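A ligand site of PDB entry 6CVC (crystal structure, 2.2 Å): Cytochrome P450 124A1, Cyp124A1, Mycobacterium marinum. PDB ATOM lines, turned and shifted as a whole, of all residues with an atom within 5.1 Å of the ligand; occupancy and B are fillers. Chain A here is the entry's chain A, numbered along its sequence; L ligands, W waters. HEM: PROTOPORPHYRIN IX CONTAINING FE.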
ATOM      1  N   SER A  86     -13.380  35.586  10.166  1.00  0.00           N
ATOM      2  CA  SER A  86     -12.140  34.824  10.175  1.00  0.00           C
ATOM      3  C   SER A  86     -10.930  35.721   9.954  1.00  0.00           C
ATOM      4  O   SER A  86      -9.838  35.426  10.451  1.00  0.00           O
ATOM      5  CB  SER A  86     -12.189  33.733   9.109  1.00  0.00           C
ATOM      6  OG  SER A  86     -13.303  32.878   9.302  1.00  0.00           O
ATOM      7  N   MET A 114      -2.665  25.152  19.573  1.00  0.00           N
ATOM      8  CA  MET A 114      -2.677  26.448  18.895  1.00  0.00           C
ATOM      9  C   MET A 114      -4.079  26.889  18.479  1.00  0.00           C
ATOM     10  O   MET A 114      -4.276  28.078  18.226  1.00  0.00           O
ATOM     11  CB  MET A 114      -1.778  26.402  17.657  1.00  0.00           C
ATOM     12  CG  MET A 114      -2.271  25.479  16.563  1.00  0.00           C
ATOM     13  SD  MET A 114      -1.184  25.441  15.126  1.00  0.00           S
ATOM     14  CE  MET A 114       0.306  24.769  15.857  1.00  0.00           C
ATOM     15  N   ILE A 115      -5.049  25.973  18.417  1.00  0.00           N
ATOM     16  CA  ILE A 115      -6.360  26.327  17.898  1.00  0.00           C
ATOM     17  C   ILE A 115      -7.176  27.167  18.882  1.00  0.00           C
ATOM     18  O   ILE A 115      -8.146  27.824  18.469  1.00  0.00           O
ATOM     19  CB  ILE A 115      -7.147  25.071  17.497  1.00  0.00           C
ATOM     20  CG1 ILE A 115      -8.129  25.388  16.362  1.00  0.00           C
ATOM     21  CG2 ILE A 115      -7.885  24.486  18.691  1.00  0.00           C
ATOM     22  CD1 ILE A 115      -8.860  24.177  15.821  1.00  0.00           C
ATOM     23  N   HIS A 122      -0.441  32.475  19.726  1.00  0.00           N
ATOM     24  CA  HIS A 122      -0.767  31.564  18.629  1.00  0.00           C
ATOM     25  C   HIS A 122       0.298  31.623  17.530  1.00  0.00           C
ATOM     26  O   HIS A 122       0.692  30.587  16.990  1.00  0.00           O
ATOM     27  CB  HIS A 122      -2.146  31.907  18.063  1.00  0.00           C
ATOM     28  CG  HIS A 122      -2.406  31.297  16.717  1.00  0.00           C
ATOM     29  ND1 HIS A 122      -2.204  31.979  15.543  1.00  0.00           N
ATOM     30  CD2 HIS A 122      -2.847  30.066  16.369  1.00  0.00           C
ATOM     31  CE1 HIS A 122      -2.513  31.200  14.519  1.00  0.00           C
ATOM     32  NE2 HIS A 122      -2.911  30.034  14.995  1.00  0.00           N
ATOM     33  N   ARG A 126       2.548  28.406  16.340  1.00  0.00           N
ATOM     34  CA  ARG A 126       2.349  27.867  15.003  1.00  0.00           C
ATOM     35  C   ARG A 126       3.590  27.998  14.137  1.00  0.00           C
ATOM     36  O   ARG A 126       3.864  27.134  13.303  1.00  0.00           O
ATOM     37  CB  ARG A 126       1.154  28.560  14.335  1.00  0.00           C
ATOM     38  CG  ARG A 126       0.960  28.171  12.872  1.00  0.00           C
ATOM     39  CD  ARG A 126      -0.448  28.463  12.393  1.00  0.00           C
ATOM     40  NE  ARG A 126      -0.621  28.050  11.006  1.00  0.00           N
ATOM     41  CZ  ARG A 126      -1.811  27.878  10.421  1.00  0.00           C
ATOM     42  NH1 ARG A 126      -2.916  28.082  11.107  1.00  0.00           N
ATOM     43  NH2 ARG A 126      -1.870  27.508   9.147  1.00  0.00           N
ATOM     44  N   MET A 183       3.969   9.895  11.140  1.00  0.00           N
ATOM     45  CA  MET A 183       4.763  11.118  11.161  1.00  0.00           C
ATOM     46  C   MET A 183       5.352  11.375  12.543  1.00  0.00           C
ATOM     47  O   MET A 183       6.430  11.988  12.647  1.00  0.00           O
ATOM     48  CB  MET A 183       3.925  12.316  10.700  1.00  0.00           C
ATOM     49  CG  MET A 183       2.930  12.849  11.725  1.00  0.00           C
ATOM     50  SD  MET A 183       2.136  14.368  11.166  1.00  0.00           S
ATOM     51  CE  MET A 183       1.246  13.786   9.731  1.00  0.00           C
ATOM     52  N   PHE A 264       0.069  19.499  21.238  1.00  0.00           N
ATOM     53  CA  PHE A 264      -0.123  19.531  19.788  1.00  0.00           C
ATOM     54  C   PHE A 264      -0.464  18.150  19.236  1.00  0.00           C
ATOM     55  O   PHE A 264      -1.227  18.049  18.271  1.00  0.00           O
ATOM     56  CB  PHE A 264       1.128  20.080  19.101  1.00  0.00           C
ATOM     57  CG  PHE A 264       1.091  19.998  17.595  1.00  0.00           C
ATOM     58  CD1 PHE A 264       0.182  20.759  16.877  1.00  0.00           C
ATOM     59  CD2 PHE A 264       1.947  19.160  16.920  1.00  0.00           C
ATOM     60  CE1 PHE A 264       0.147  20.681  15.498  1.00  0.00           C
ATOM     61  CE2 PHE A 264       1.913  19.076  15.532  1.00  0.00           C
ATOM     62  CZ  PHE A 264       1.012  19.839  14.826  1.00  0.00           C
ATOM     63  N   LEU A 267      -4.086  17.568  19.774  1.00  0.00           N
ATOM     64  CA  LEU A 267      -4.881  18.296  18.793  1.00  0.00           C
ATOM     65  C   LEU A 267      -4.924  17.556  17.454  1.00  0.00           C
ATOM     66  O   LEU A 267      -5.966  17.534  16.790  1.00  0.00           O
ATOM     67  CB  LEU A 267      -4.300  19.701  18.600  1.00  0.00           C
ATOM     68  CG  LEU A 267      -4.899  20.545  17.461  1.00  0.00           C
ATOM     69  CD1 LEU A 267      -6.350  20.910  17.769  1.00  0.00           C
ATOM     70  CD2 LEU A 267      -4.068  21.791  17.213  1.00  0.00           C
ATOM     71  N   LEU A 268      -3.804  16.937  17.069  1.00  0.00           N
ATOM     72  CA  LEU A 268      -3.763  16.249  15.777  1.00  0.00           C
ATOM     73  C   LEU A 268      -4.660  15.026  15.757  1.00  0.00           C
ATOM     74  O   LEU A 268      -5.388  14.803  14.777  1.00  0.00           O
ATOM     75  CB  LEU A 268      -2.322  15.859  15.436  1.00  0.00           C
ATOM     76  CG  LEU A 268      -1.364  16.979  15.031  1.00  0.00           C
ATOM     77  CD1 LEU A 268      -0.074  16.390  14.492  1.00  0.00           C
ATOM     78  CD2 LEU A 268      -2.018  17.890  13.999  1.00  0.00           C
ATOM     79  N   ALA A 271      -8.346  16.975  15.657  1.00  0.00           N
ATOM     80  CA  ALA A 271      -8.601  17.921  14.571  1.00  0.00           C
ATOM     81  C   ALA A 271      -8.045  17.434  13.228  1.00  0.00           C
ATOM     82  O   ALA A 271      -8.526  17.883  12.189  1.00  0.00           O
ATOM     83  CB  ALA A 271      -8.007  19.287  14.909  1.00  0.00           C
ATOM     84  N   GLY A 272      -7.051  16.553  13.240  1.00  0.00           N
ATOM     85  CA  GLY A 272      -6.486  16.061  11.995  1.00  0.00           C
ATOM     86  C   GLY A 272      -6.837  14.617  11.716  1.00  0.00           C
ATOM     87  O   GLY A 272      -6.206  13.966  10.869  1.00  0.00           O
ATOM     88  N   THR A 275     -11.745  14.673  11.104  1.00  0.00           N
ATOM     89  CA  THR A 275     -12.083  15.573  10.003  1.00  0.00           C
ATOM     90  C   THR A 275     -11.862  14.891   8.665  1.00  0.00           C
ATOM     91  O   THR A 275     -12.775  14.834   7.824  1.00  0.00           O
ATOM     92  CB  THR A 275     -11.257  16.860  10.106  1.00  0.00           C
ATOM     93  OG1 THR A 275      -9.867  16.535  10.180  1.00  0.00           O
ATOM     94  CG2 THR A 275     -11.659  17.647  11.339  1.00  0.00           C
ATOM     95  N   THR A 276     -10.649  14.374   8.428  1.00  0.00           N
ATOM     96  CA  THR A 276     -10.382  13.663   7.183  1.00  0.00           C
ATOM     97  C   THR A 276     -11.230  12.395   7.066  1.00  0.00           C
ATOM     98  O   THR A 276     -11.635  12.022   5.962  1.00  0.00           O
ATOM     99  CB  THR A 276      -8.892  13.301   7.089  1.00  0.00           C
ATOM    100  OG1 THR A 276      -8.105  14.489   7.249  1.00  0.00           O
ATOM    101  CG2 THR A 276      -8.573  12.666   5.756  1.00  0.00           C
ATOM    102  N   ALA A 279     -14.586  13.442   5.797  1.00  0.00           N
ATOM    103  CA  ALA A 279     -14.458  13.887   4.419  1.00  0.00           C
ATOM    104  C   ALA A 279     -14.411  12.707   3.464  1.00  0.00           C
ATOM    105  O   ALA A 279     -14.957  12.757   2.357  1.00  0.00           O
ATOM    106  CB  ALA A 279     -13.221  14.763   4.260  1.00  0.00           C
ATOM    107  N   VAL A 313     -14.699  18.364  -0.040  1.00  0.00           N
ATOM    108  CA  VAL A 313     -14.604  19.126   1.209  1.00  0.00           C
ATOM    109  C   VAL A 313     -15.777  20.102   1.334  1.00  0.00           C
ATOM    110  O   VAL A 313     -16.351  20.252   2.422  1.00  0.00           O
ATOM    111  CB  VAL A 313     -13.256  19.848   1.296  1.00  0.00           C
ATOM    112  CG1 VAL A 313     -13.176  20.689   2.554  1.00  0.00           C
ATOM    113  CG2 VAL A 313     -12.117  18.838   1.259  1.00  0.00           C
ATOM    114  N   PRO A 318     -16.600  18.700   6.948  1.00  0.00           N
ATOM    115  CA  PRO A 318     -16.460  17.851   8.153  1.00  0.00           C
ATOM    116  C   PRO A 318     -16.567  18.635   9.451  1.00  0.00           C
ATOM    117  O   PRO A 318     -17.148  18.128  10.423  1.00  0.00           O
ATOM    118  CB  PRO A 318     -15.062  17.227   7.975  1.00  0.00           C
ATOM    119  CG  PRO A 318     -14.813  17.286   6.504  1.00  0.00           C
ATOM    120  CD  PRO A 318     -15.449  18.549   6.034  1.00  0.00           C
ATOM    121  N   VAL A 319     -16.035  19.847   9.489  1.00  0.00           N
ATOM    122  CA  VAL A 319     -16.197  20.727  10.640  1.00  0.00           C
ATOM    123  C   VAL A 319     -17.444  21.569  10.393  1.00  0.00           C
ATOM    124  O   VAL A 319     -17.467  22.408   9.489  1.00  0.00           O
ATOM    125  CB  VAL A 319     -14.959  21.607  10.868  1.00  0.00           C
ATOM    126  CG1 VAL A 319     -15.222  22.612  11.968  1.00  0.00           C
ATOM    127  CG2 VAL A 319     -13.755  20.735  11.200  1.00  0.00           C
ATOM    128  N   MET A 322     -17.175  26.661  13.890  1.00  0.00           N
ATOM    129  CA  MET A 322     -16.106  27.041  14.807  1.00  0.00           C
ATOM    130  C   MET A 322     -16.573  28.262  15.579  1.00  0.00           C
ATOM    131  O   MET A 322     -17.117  29.205  14.985  1.00  0.00           O
ATOM    132  CB  MET A 322     -14.802  27.344  14.064  1.00  0.00           C
ATOM    133  CG  MET A 322     -13.996  26.110  13.673  1.00  0.00           C
ATOM    134  SD  MET A 322     -13.314  25.241  15.095  1.00  0.00           S
ATOM    135  CE  MET A 322     -12.458  23.894  14.296  1.00  0.00           C
ATOM    136  N   ARG A 324     -16.238  31.627  18.092  1.00  0.00           N
ATOM    137  CA  ARG A 324     -15.387  32.763  18.396  1.00  0.00           C
ATOM    138  C   ARG A 324     -15.997  33.536  19.558  1.00  0.00           C
ATOM    139  O   ARG A 324     -17.197  33.446  19.839  1.00  0.00           O
ATOM    140  CB  ARG A 324     -15.207  33.682  17.180  1.00  0.00           C
ATOM    141  CG  ARG A 324     -14.455  33.058  16.022  1.00  0.00           C
ATOM    142  CD  ARG A 324     -13.001  32.799  16.380  1.00  0.00           C
ATOM    143  NE  ARG A 324     -12.211  32.392  15.211  1.00  0.00           N
ATOM    144  CZ  ARG A 324     -11.962  31.131  14.877  1.00  0.00           C
ATOM    145  NH1 ARG A 324     -12.440  30.134  15.618  1.00  0.00           N
ATOM    146  NH2 ARG A 324     -11.241  30.860  13.807  1.00  0.00           N
ATOM    147  N   TYR A 347     -19.695  26.678   8.779  1.00  0.00           N
ATOM    148  CA  TYR A 347     -19.140  26.375   7.464  1.00  0.00           C
ATOM    149  C   TYR A 347     -20.097  25.521   6.636  1.00  0.00           C
ATOM    150  O   TYR A 347     -20.066  25.585   5.400  1.00  0.00           O
ATOM    151  CB  TYR A 347     -17.801  25.669   7.613  1.00  0.00           C
ATOM    152  CG  TYR A 347     -16.826  26.384   8.516  1.00  0.00           C
ATOM    153  CD1 TYR A 347     -16.330  27.640   8.195  1.00  0.00           C
ATOM    154  CD2 TYR A 347     -16.378  25.788   9.701  1.00  0.00           C
ATOM    155  CE1 TYR A 347     -15.446  28.292   9.022  1.00  0.00           C
ATOM    156  CE2 TYR A 347     -15.485  26.436  10.531  1.00  0.00           C
ATOM    157  CZ  TYR A 347     -15.019  27.685  10.187  1.00  0.00           C
ATOM    158  OH  TYR A 347     -14.127  28.333  11.017  1.00  0.00           O
ATOM    159  N   GLY A 374     -14.464  24.826   3.991  1.00  0.00           N
ATOM    160  CA  GLY A 374     -14.404  23.641   4.828  1.00  0.00           C
ATOM    161  C   GLY A 374     -13.195  23.622   5.745  1.00  0.00           C
ATOM    162  O   GLY A 374     -13.263  23.092   6.850  1.00  0.00           O
ATOM    163  N   PHE A 375     -12.091  24.208   5.291  1.00  0.00           N
ATOM    164  CA  PHE A 375     -10.904  24.388   6.119  1.00  0.00           C
ATOM    165  C   PHE A 375     -10.940  25.704   6.886  1.00  0.00           C
ATOM    166  O   PHE A 375      -9.907  26.118   7.426  1.00  0.00           O
ATOM    167  CB  PHE A 375      -9.643  24.331   5.263  1.00  0.00           C
ATOM    168  CG  PHE A 375      -9.450  23.020   4.543  1.00  0.00           C
ATOM    169  CD1 PHE A 375      -9.213  21.853   5.257  1.00  0.00           C
ATOM    170  CD2 PHE A 375      -9.499  22.962   3.162  1.00  0.00           C
ATOM    171  CE1 PHE A 375      -9.040  20.653   4.597  1.00  0.00           C
ATOM    172  CE2 PHE A 375      -9.317  21.759   2.505  1.00  0.00           C
ATOM    173  CZ  PHE A 375      -9.090  20.601   3.224  1.00  0.00           C
ATOM    174  N   GLY A 376     -12.091  26.360   6.951  1.00  0.00           N
ATOM    175  CA  GLY A 376     -12.213  27.655   7.581  1.00  0.00           C
ATOM    176  C   GLY A 376     -12.266  28.788   6.565  1.00  0.00           C
ATOM    177  O   GLY A 376     -11.993  28.623   5.374  1.00  0.00           O
ATOM    178  N   GLY A 377     -12.618  29.971   7.066  1.00  0.00           N
ATOM    179  CA  GLY A 377     -12.718  31.143   6.232  1.00  0.00           C
ATOM    180  C   GLY A 377     -11.417  31.822   5.882  1.00  0.00           C
ATOM    181  O   GLY A 377     -11.438  32.942   5.371  1.00  0.00           O
ATOM    182  N   GLY A 378     -10.281  31.183   6.136  1.00  0.00           N
ATOM    183  CA  GLY A 378      -8.986  31.791   5.911  1.00  0.00           C
ATOM    184  C   GLY A 378      -8.539  32.642   7.080  1.00  0.00           C
ATOM    185  O   GLY A 378      -9.293  32.956   8.004  1.00  0.00           O
ATOM    186  N   ALA A 380      -5.645  33.622  10.229  1.00  0.00           N
ATOM    187  CA  ALA A 380      -4.569  33.192  11.125  1.00  0.00           C
ATOM    188  C   ALA A 380      -4.676  31.704  11.462  1.00  0.00           C
ATOM    189  O   ALA A 380      -3.661  31.013  11.511  1.00  0.00           O
ATOM    190  CB  ALA A 380      -4.589  34.032  12.409  1.00  0.00           C
ATOM    191  N   HIS A 381      -5.887  31.210  11.683  1.00  0.00           N
ATOM    192  CA  HIS A 381      -6.101  29.840  12.137  1.00  0.00           C
ATOM    193  C   HIS A 381      -6.418  28.881  10.987  1.00  0.00           C
ATOM    194  O   HIS A 381      -6.950  27.800  11.234  1.00  0.00           O
ATOM    195  CB  HIS A 381      -7.219  29.788  13.167  1.00  0.00           C
ATOM    196  CG  HIS A 381      -6.880  30.442  14.470  1.00  0.00           C
ATOM    197  ND1 HIS A 381      -6.334  29.756  15.530  1.00  0.00           N
ATOM    198  CD2 HIS A 381      -6.996  31.729  14.882  1.00  0.00           C
ATOM    199  CE1 HIS A 381      -6.138  30.582  16.538  1.00  0.00           C
ATOM    200  NE2 HIS A 381      -6.526  31.784  16.164  1.00  0.00           N
ATOM    201  N   PHE A 382      -6.095  29.258   9.752  1.00  0.00           N
ATOM    202  CA  PHE A 382      -6.388  28.396   8.617  1.00  0.00           C
ATOM    203  C   PHE A 382      -5.738  27.029   8.798  1.00  0.00           C
ATOM    204  O   PHE A 382      -4.602  26.924   9.266  1.00  0.00           O
ATOM    205  CB  PHE A 382      -5.919  29.031   7.308  1.00  0.00           C
ATOM    206  CG  PHE A 382      -6.165  28.169   6.106  1.00  0.00           C
ATOM    207  CD1 PHE A 382      -7.432  28.043   5.568  1.00  0.00           C
ATOM    208  CD2 PHE A 382      -5.130  27.455   5.525  1.00  0.00           C
ATOM    209  CE1 PHE A 382      -7.666  27.243   4.470  1.00  0.00           C
ATOM    210  CE2 PHE A 382      -5.350  26.654   4.418  1.00  0.00           C
ATOM    211  CZ  PHE A 382      -6.623  26.555   3.898  1.00  0.00           C
ATOM    212  N   CYS A 383      -6.481  25.978   8.417  1.00  0.00           N
ATOM    213  CA  CYS A 383      -6.106  24.597   8.711  1.00  0.00           C
ATOM    214  C   CYS A 383      -4.663  24.313   8.329  1.00  0.00           C
ATOM    215  O   CYS A 383      -4.288  24.411   7.164  1.00  0.00           O
ATOM    216  CB  CYS A 383      -7.048  23.645   7.980  1.00  0.00           C
ATOM    217  SG  CYS A 383      -6.691  21.902   8.281  1.00  0.00           S
ATOM    218  N   LEU A 384      -3.862  23.946   9.337  1.00  0.00           N
ATOM    219  CA  LEU A 384      -2.442  23.687   9.114  1.00  0.00           C
ATOM    220  C   LEU A 384      -2.215  22.503   8.190  1.00  0.00           C
ATOM    221  O   LEU A 384      -1.237  22.483   7.438  1.00  0.00           O
ATOM    222  CB  LEU A 384      -1.744  23.466  10.458  1.00  0.00           C
ATOM    223  CG  LEU A 384      -0.231  23.250  10.441  1.00  0.00           C
ATOM    224  CD1 LEU A 384       0.488  24.523  10.025  1.00  0.00           C
ATOM    225  CD2 LEU A 384       0.253  22.779  11.800  1.00  0.00           C
ATOM    226  N   GLY A 385      -3.102  21.514   8.229  1.00  0.00           N
ATOM    227  CA  GLY A 385      -2.942  20.334   7.402  1.00  0.00           C
ATOM    228  C   GLY A 385      -3.917  20.269   6.242  1.00  0.00           C
ATOM    229  O   GLY A 385      -4.333  19.182   5.832  1.00  0.00           O
ATOM    230  N   ALA A 386      -4.299  21.430   5.706  1.00  0.00           N
ATOM    231  CA  ALA A 386      -5.283  21.471   4.634  1.00  0.00           C
ATOM    232  C   ALA A 386      -4.801  20.713   3.403  1.00  0.00           C
ATOM    233  O   ALA A 386      -5.532  19.875   2.857  1.00  0.00           O
ATOM    234  CB  ALA A 386      -5.604  22.926   4.276  1.00  0.00           C
ATOM    235  N   LEU A 388      -2.407  18.479   3.330  1.00  0.00           N
ATOM    236  CA  LEU A 388      -2.286  17.084   3.713  1.00  0.00           C
ATOM    237  C   LEU A 388      -3.646  16.391   3.666  1.00  0.00           C
ATOM    238  O   LEU A 388      -3.756  15.252   3.199  1.00  0.00           O
ATOM    239  CB  LEU A 388      -1.671  16.956   5.110  1.00  0.00           C
ATOM    240  CG  LEU A 388      -1.625  15.544   5.684  1.00  0.00           C
ATOM    241  CD1 LEU A 388      -0.863  14.605   4.768  1.00  0.00           C
ATOM    242  CD2 LEU A 388      -1.007  15.556   7.078  1.00  0.00           C
ATOM    243  N   ALA A 389      -4.698  17.078   4.132  1.00  0.00           N
ATOM    244  CA  ALA A 389      -6.043  16.519   4.039  1.00  0.00           C
ATOM    245  C   ALA A 389      -6.442  16.298   2.583  1.00  0.00           C
ATOM    246  O   ALA A 389      -7.040  15.274   2.247  1.00  0.00           O
ATOM    247  CB  ALA A 389      -7.037  17.454   4.736  1.00  0.00           C
ATOM    248  N   GLU A 392      -4.708  13.197   1.472  1.00  0.00           N
ATOM    249  CA  GLU A 392      -5.317  11.988   2.012  1.00  0.00           C
ATOM    250  C   GLU A 392      -6.609  11.640   1.278  1.00  0.00           C
ATOM    251  O   GLU A 392      -6.878  10.472   1.003  1.00  0.00           O
ATOM    252  CB  GLU A 392      -5.577  12.147   3.514  1.00  0.00           C
ATOM    253  CG  GLU A 392      -4.315  12.348   4.347  1.00  0.00           C
ATOM    254  CD  GLU A 392      -4.613  12.650   5.805  1.00  0.00           C
ATOM    255  OE1 GLU A 392      -3.967  12.048   6.682  1.00  0.00           O
ATOM    256  OE2 GLU A 392      -5.478  13.501   6.071  1.00  0.00           O
ATOM    257  N   ILE A 393      -7.406  12.660   0.941  1.00  0.00           N
ATOM    258  CA  ILE A 393      -8.640  12.419   0.206  1.00  0.00           C
ATOM    259  C   ILE A 393      -8.339  11.898  -1.199  1.00  0.00           C
ATOM    260  O   ILE A 393      -8.977  10.943  -1.664  1.00  0.00           O
ATOM    261  CB  ILE A 393      -9.503  13.696   0.165  1.00  0.00           C
ATOM    262  CG1 ILE A 393      -9.916  14.099   1.584  1.00  0.00           C
ATOM    263  CG2 ILE A 393     -10.729  13.484  -0.718  1.00  0.00           C
ATOM    264  CD1 ILE A 393     -10.578  15.456   1.654  1.00  0.00           C
HETATM  265  CHA HEM L   1      -7.617  24.087  11.949  1.00  0.00           C
HETATM  266  CHB HEM L   1     -10.849  21.740   9.192  1.00  0.00           C
HETATM  267  CHC HEM L   1      -7.644  18.203   8.372  1.00  0.00           C
HETATM  268  CHD HEM L   1      -4.564  20.337  11.468  1.00  0.00           C
HETATM  269  C1A HEM L   1      -8.768  23.776  11.252  1.00  0.00           C
HETATM  270  C2A HEM L   1      -9.961  24.600  11.151  1.00  0.00           C
HETATM  271  C3A HEM L   1     -10.846  23.949  10.394  1.00  0.00           C
HETATM  272  C4A HEM L   1     -10.258  22.695   9.982  1.00  0.00           C
HETATM  273  CMA HEM L   1     -12.265  24.431  10.009  1.00  0.00           C
HETATM  274  CAA HEM L   1     -10.159  25.985  11.813  1.00  0.00           C
HETATM  275  CBA HEM L   1      -9.977  27.063  10.747  1.00  0.00           C
HETATM  276  CGA HEM L   1     -10.184  28.431  11.348  1.00  0.00           C
HETATM  277  O1A HEM L   1     -10.423  28.519  12.577  1.00  0.00           O
HETATM  278  O2A HEM L   1     -10.109  29.433  10.589  1.00  0.00           O
HETATM  279  C1B HEM L   1     -10.255  20.611   8.683  1.00  0.00           C
HETATM  280  C2B HEM L   1     -10.826  19.710   7.708  1.00  0.00           C
HETATM  281  C3B HEM L   1      -9.938  18.719   7.471  1.00  0.00           C
HETATM  282  C4B HEM L   1      -8.781  18.974   8.309  1.00  0.00           C
HETATM  283  CMB HEM L   1     -12.225  19.931   7.086  1.00  0.00           C
HETATM  284  CAB HEM L   1     -10.035  17.497   6.516  1.00  0.00           C
HETATM  285  CBB HEM L   1     -11.034  17.273   5.651  1.00  0.00           C
HETATM  286  C1C HEM L   1      -6.520  18.471   9.128  1.00  0.00           C
HETATM  287  C2C HEM L   1      -5.305  17.682   9.175  1.00  0.00           C
HETATM  288  C3C HEM L   1      -4.446  18.276  10.035  1.00  0.00           C
HETATM  289  C4C HEM L   1      -5.105  19.453  10.557  1.00  0.00           C
HETATM  290  CMC HEM L   1      -5.097  16.390   8.339  1.00  0.00           C
HETATM  291  CAC HEM L   1      -3.010  17.874  10.466  1.00  0.00           C
HETATM  292  CBC HEM L   1      -2.371  16.774  10.060  1.00  0.00           C
HETATM  293  C1D HEM L   1      -5.130  21.522  11.899  1.00  0.00           C
HETATM  294  C2D HEM L   1      -4.582  22.428  12.880  1.00  0.00           C
HETATM  295  C3D HEM L   1      -5.416  23.459  13.015  1.00  0.00           C
HETATM  296  C4D HEM L   1      -6.534  23.251  12.118  1.00  0.00           C
HETATM  297  CMD HEM L   1      -3.250  22.225  13.649  1.00  0.00           C
HETATM  298  CAD HEM L   1      -5.237  24.676  13.958  1.00  0.00           C
HETATM  299  CBD HEM L   1      -4.391  25.735  13.249  1.00  0.00           C
HETATM  300  CGD HEM L   1      -4.487  27.048  13.989  1.00  0.00           C
HETATM  301  O1D HEM L   1      -5.291  27.141  14.949  1.00  0.00           O
HETATM  302  O2D HEM L   1      -3.758  27.997  13.608  1.00  0.00           O
HETATM  303  NA  HEM L   1      -8.985  22.624  10.525  1.00  0.00           N
HETATM  304  NB  HEM L   1      -9.003  20.131   9.026  1.00  0.00           N
HETATM  305  NC  HEM L   1      -6.364  19.542   9.993  1.00  0.00           N
HETATM  306  ND  HEM L   1      -6.319  22.058  11.445  1.00  0.00           N
HETATM  307 FE   HEM L   1      -7.644  21.107  10.218  1.00  0.00          FE
HETATM  308  O   HOH W   1     -11.188  27.688  14.942  1.00  0.00           O
HETATM  309  O   HOH W   2     -12.651  30.409   9.935  1.00  0.00           O
HETATM  310  O   HOH W   3      -9.429  29.222   7.842  1.00  0.00           O
HETATM  311  O   HOH W   4      -9.376  20.392  12.160  1.00  0.00           O
HETATM  312  O   HOH W   5      -8.526  31.809  10.851  1.00  0.00           O
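SG of Cys 383 binds FE of the ligand (2.3 Å). An oxygen (O1A) of the ligand lies within salt-bridge range of the guanidinium group (NH2) of Arg 324 (2.8 Å). An oxygen (O2D) of the ligand lies within salt-bridge range of the guanidinium group (NH1) of Arg 126. A ring nitrogen (ND1) of His 381 is in hydrogen-bond range of an oxygen (O1D) of the ligand, 2.9 Å away. O2D of the ligand is in hydrogen-bond range of NE2 of His 122, 2.6 Å away.
N of Gly 385 sits close to SG of Cys 383 (3.6 Å). The side-chain hydroxyl (OG1) of Thr 275 sits at hydrogen-bond distance from the backbone carbonyl oxygen (O) of Ala 271, at 2.8 Å. SG of Cys 383 sits close to N of Ala 386 (3.5 Å). ND1 of His 381 lies within hydrogen-bond range of NE2 of His 122 (3.5 Å). The backbone carbonyl oxygen (O) of Phe 382 lies within hydrogen-bond range of the guanidinium group (NH1) of Arg 126 (2.8 Å). NH1 of Arg 126 lies within hydrogen-bond range of O of Ala 380, at 3.1 Å. OG1 of Thr 276 sits at hydrogen-bond distance from OE2 of Glu 392, at 3.0 Å.
O of Ala 271 lies close to NC of the ligand (3.5 Å). Merely in contact with the ligand: Ile 115, Thr 275, Gly 374, Phe 375, Gly 272, Ala 389, Leu 388, Met 114, Ala 279, Gly 376, Thr 276, Pro 318, Gly 385, Leu 268, Val 319, Ala 380, Leu 267, Glu 392, Leu 384, Tyr 347 and Met 322. Hydrophobic or aromatic side chains that line the ligand: Met 114, Ile 115, His 122, Leu 267, Leu 268, Ala 279, Pro 318, Val 319, Met 322, Tyr 347, Phe 375, His 381, Leu 384, Leu 388 and Ala 389. Within 4 Å of the ligand: Met 114, Ile 115, His 122, Arg 126, Leu 267, Leu 268, Ala 271, Gly 272, Thr 275, Thr 276, Ala 279, Pro 318, Val 319, Met 322, Arg 324, Tyr 347, Gly 374, Phe 375, Gly 376, Ala 380, His 381, Cys 383, Leu 384, Gly 385, Leu 388, Ala 389 and Glu 392.
Water W1 lies within hydrogen-bond range of O1A of the ligand (2.6 Å), NH1 of Arg 324 (2.8 Å) and SD of Met 322 (3.2 Å). Water W2 lies within hydrogen-bond range of the side-chain hydroxyl of Ser 86, the side-chain hydroxyl of Tyr 347, an oxygen (O2A) of the ligand and the backbone NH of Gly 377. Water W3 lies within hydrogen-bond range of the backbone NH (N) of Gly 378, an oxygen (O2A) of the ligand, the backbone carbonyl oxygen (O) of Phe 375 and the backbone NH (N) of Gly 377. Water W5 lies within hydrogen-bond range of N of His 381 (2.8 Å), O2A of the ligand (2.9 Å), O of Gly 378 (3.2 Å) and N of Ala 380 (3.5 Å).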
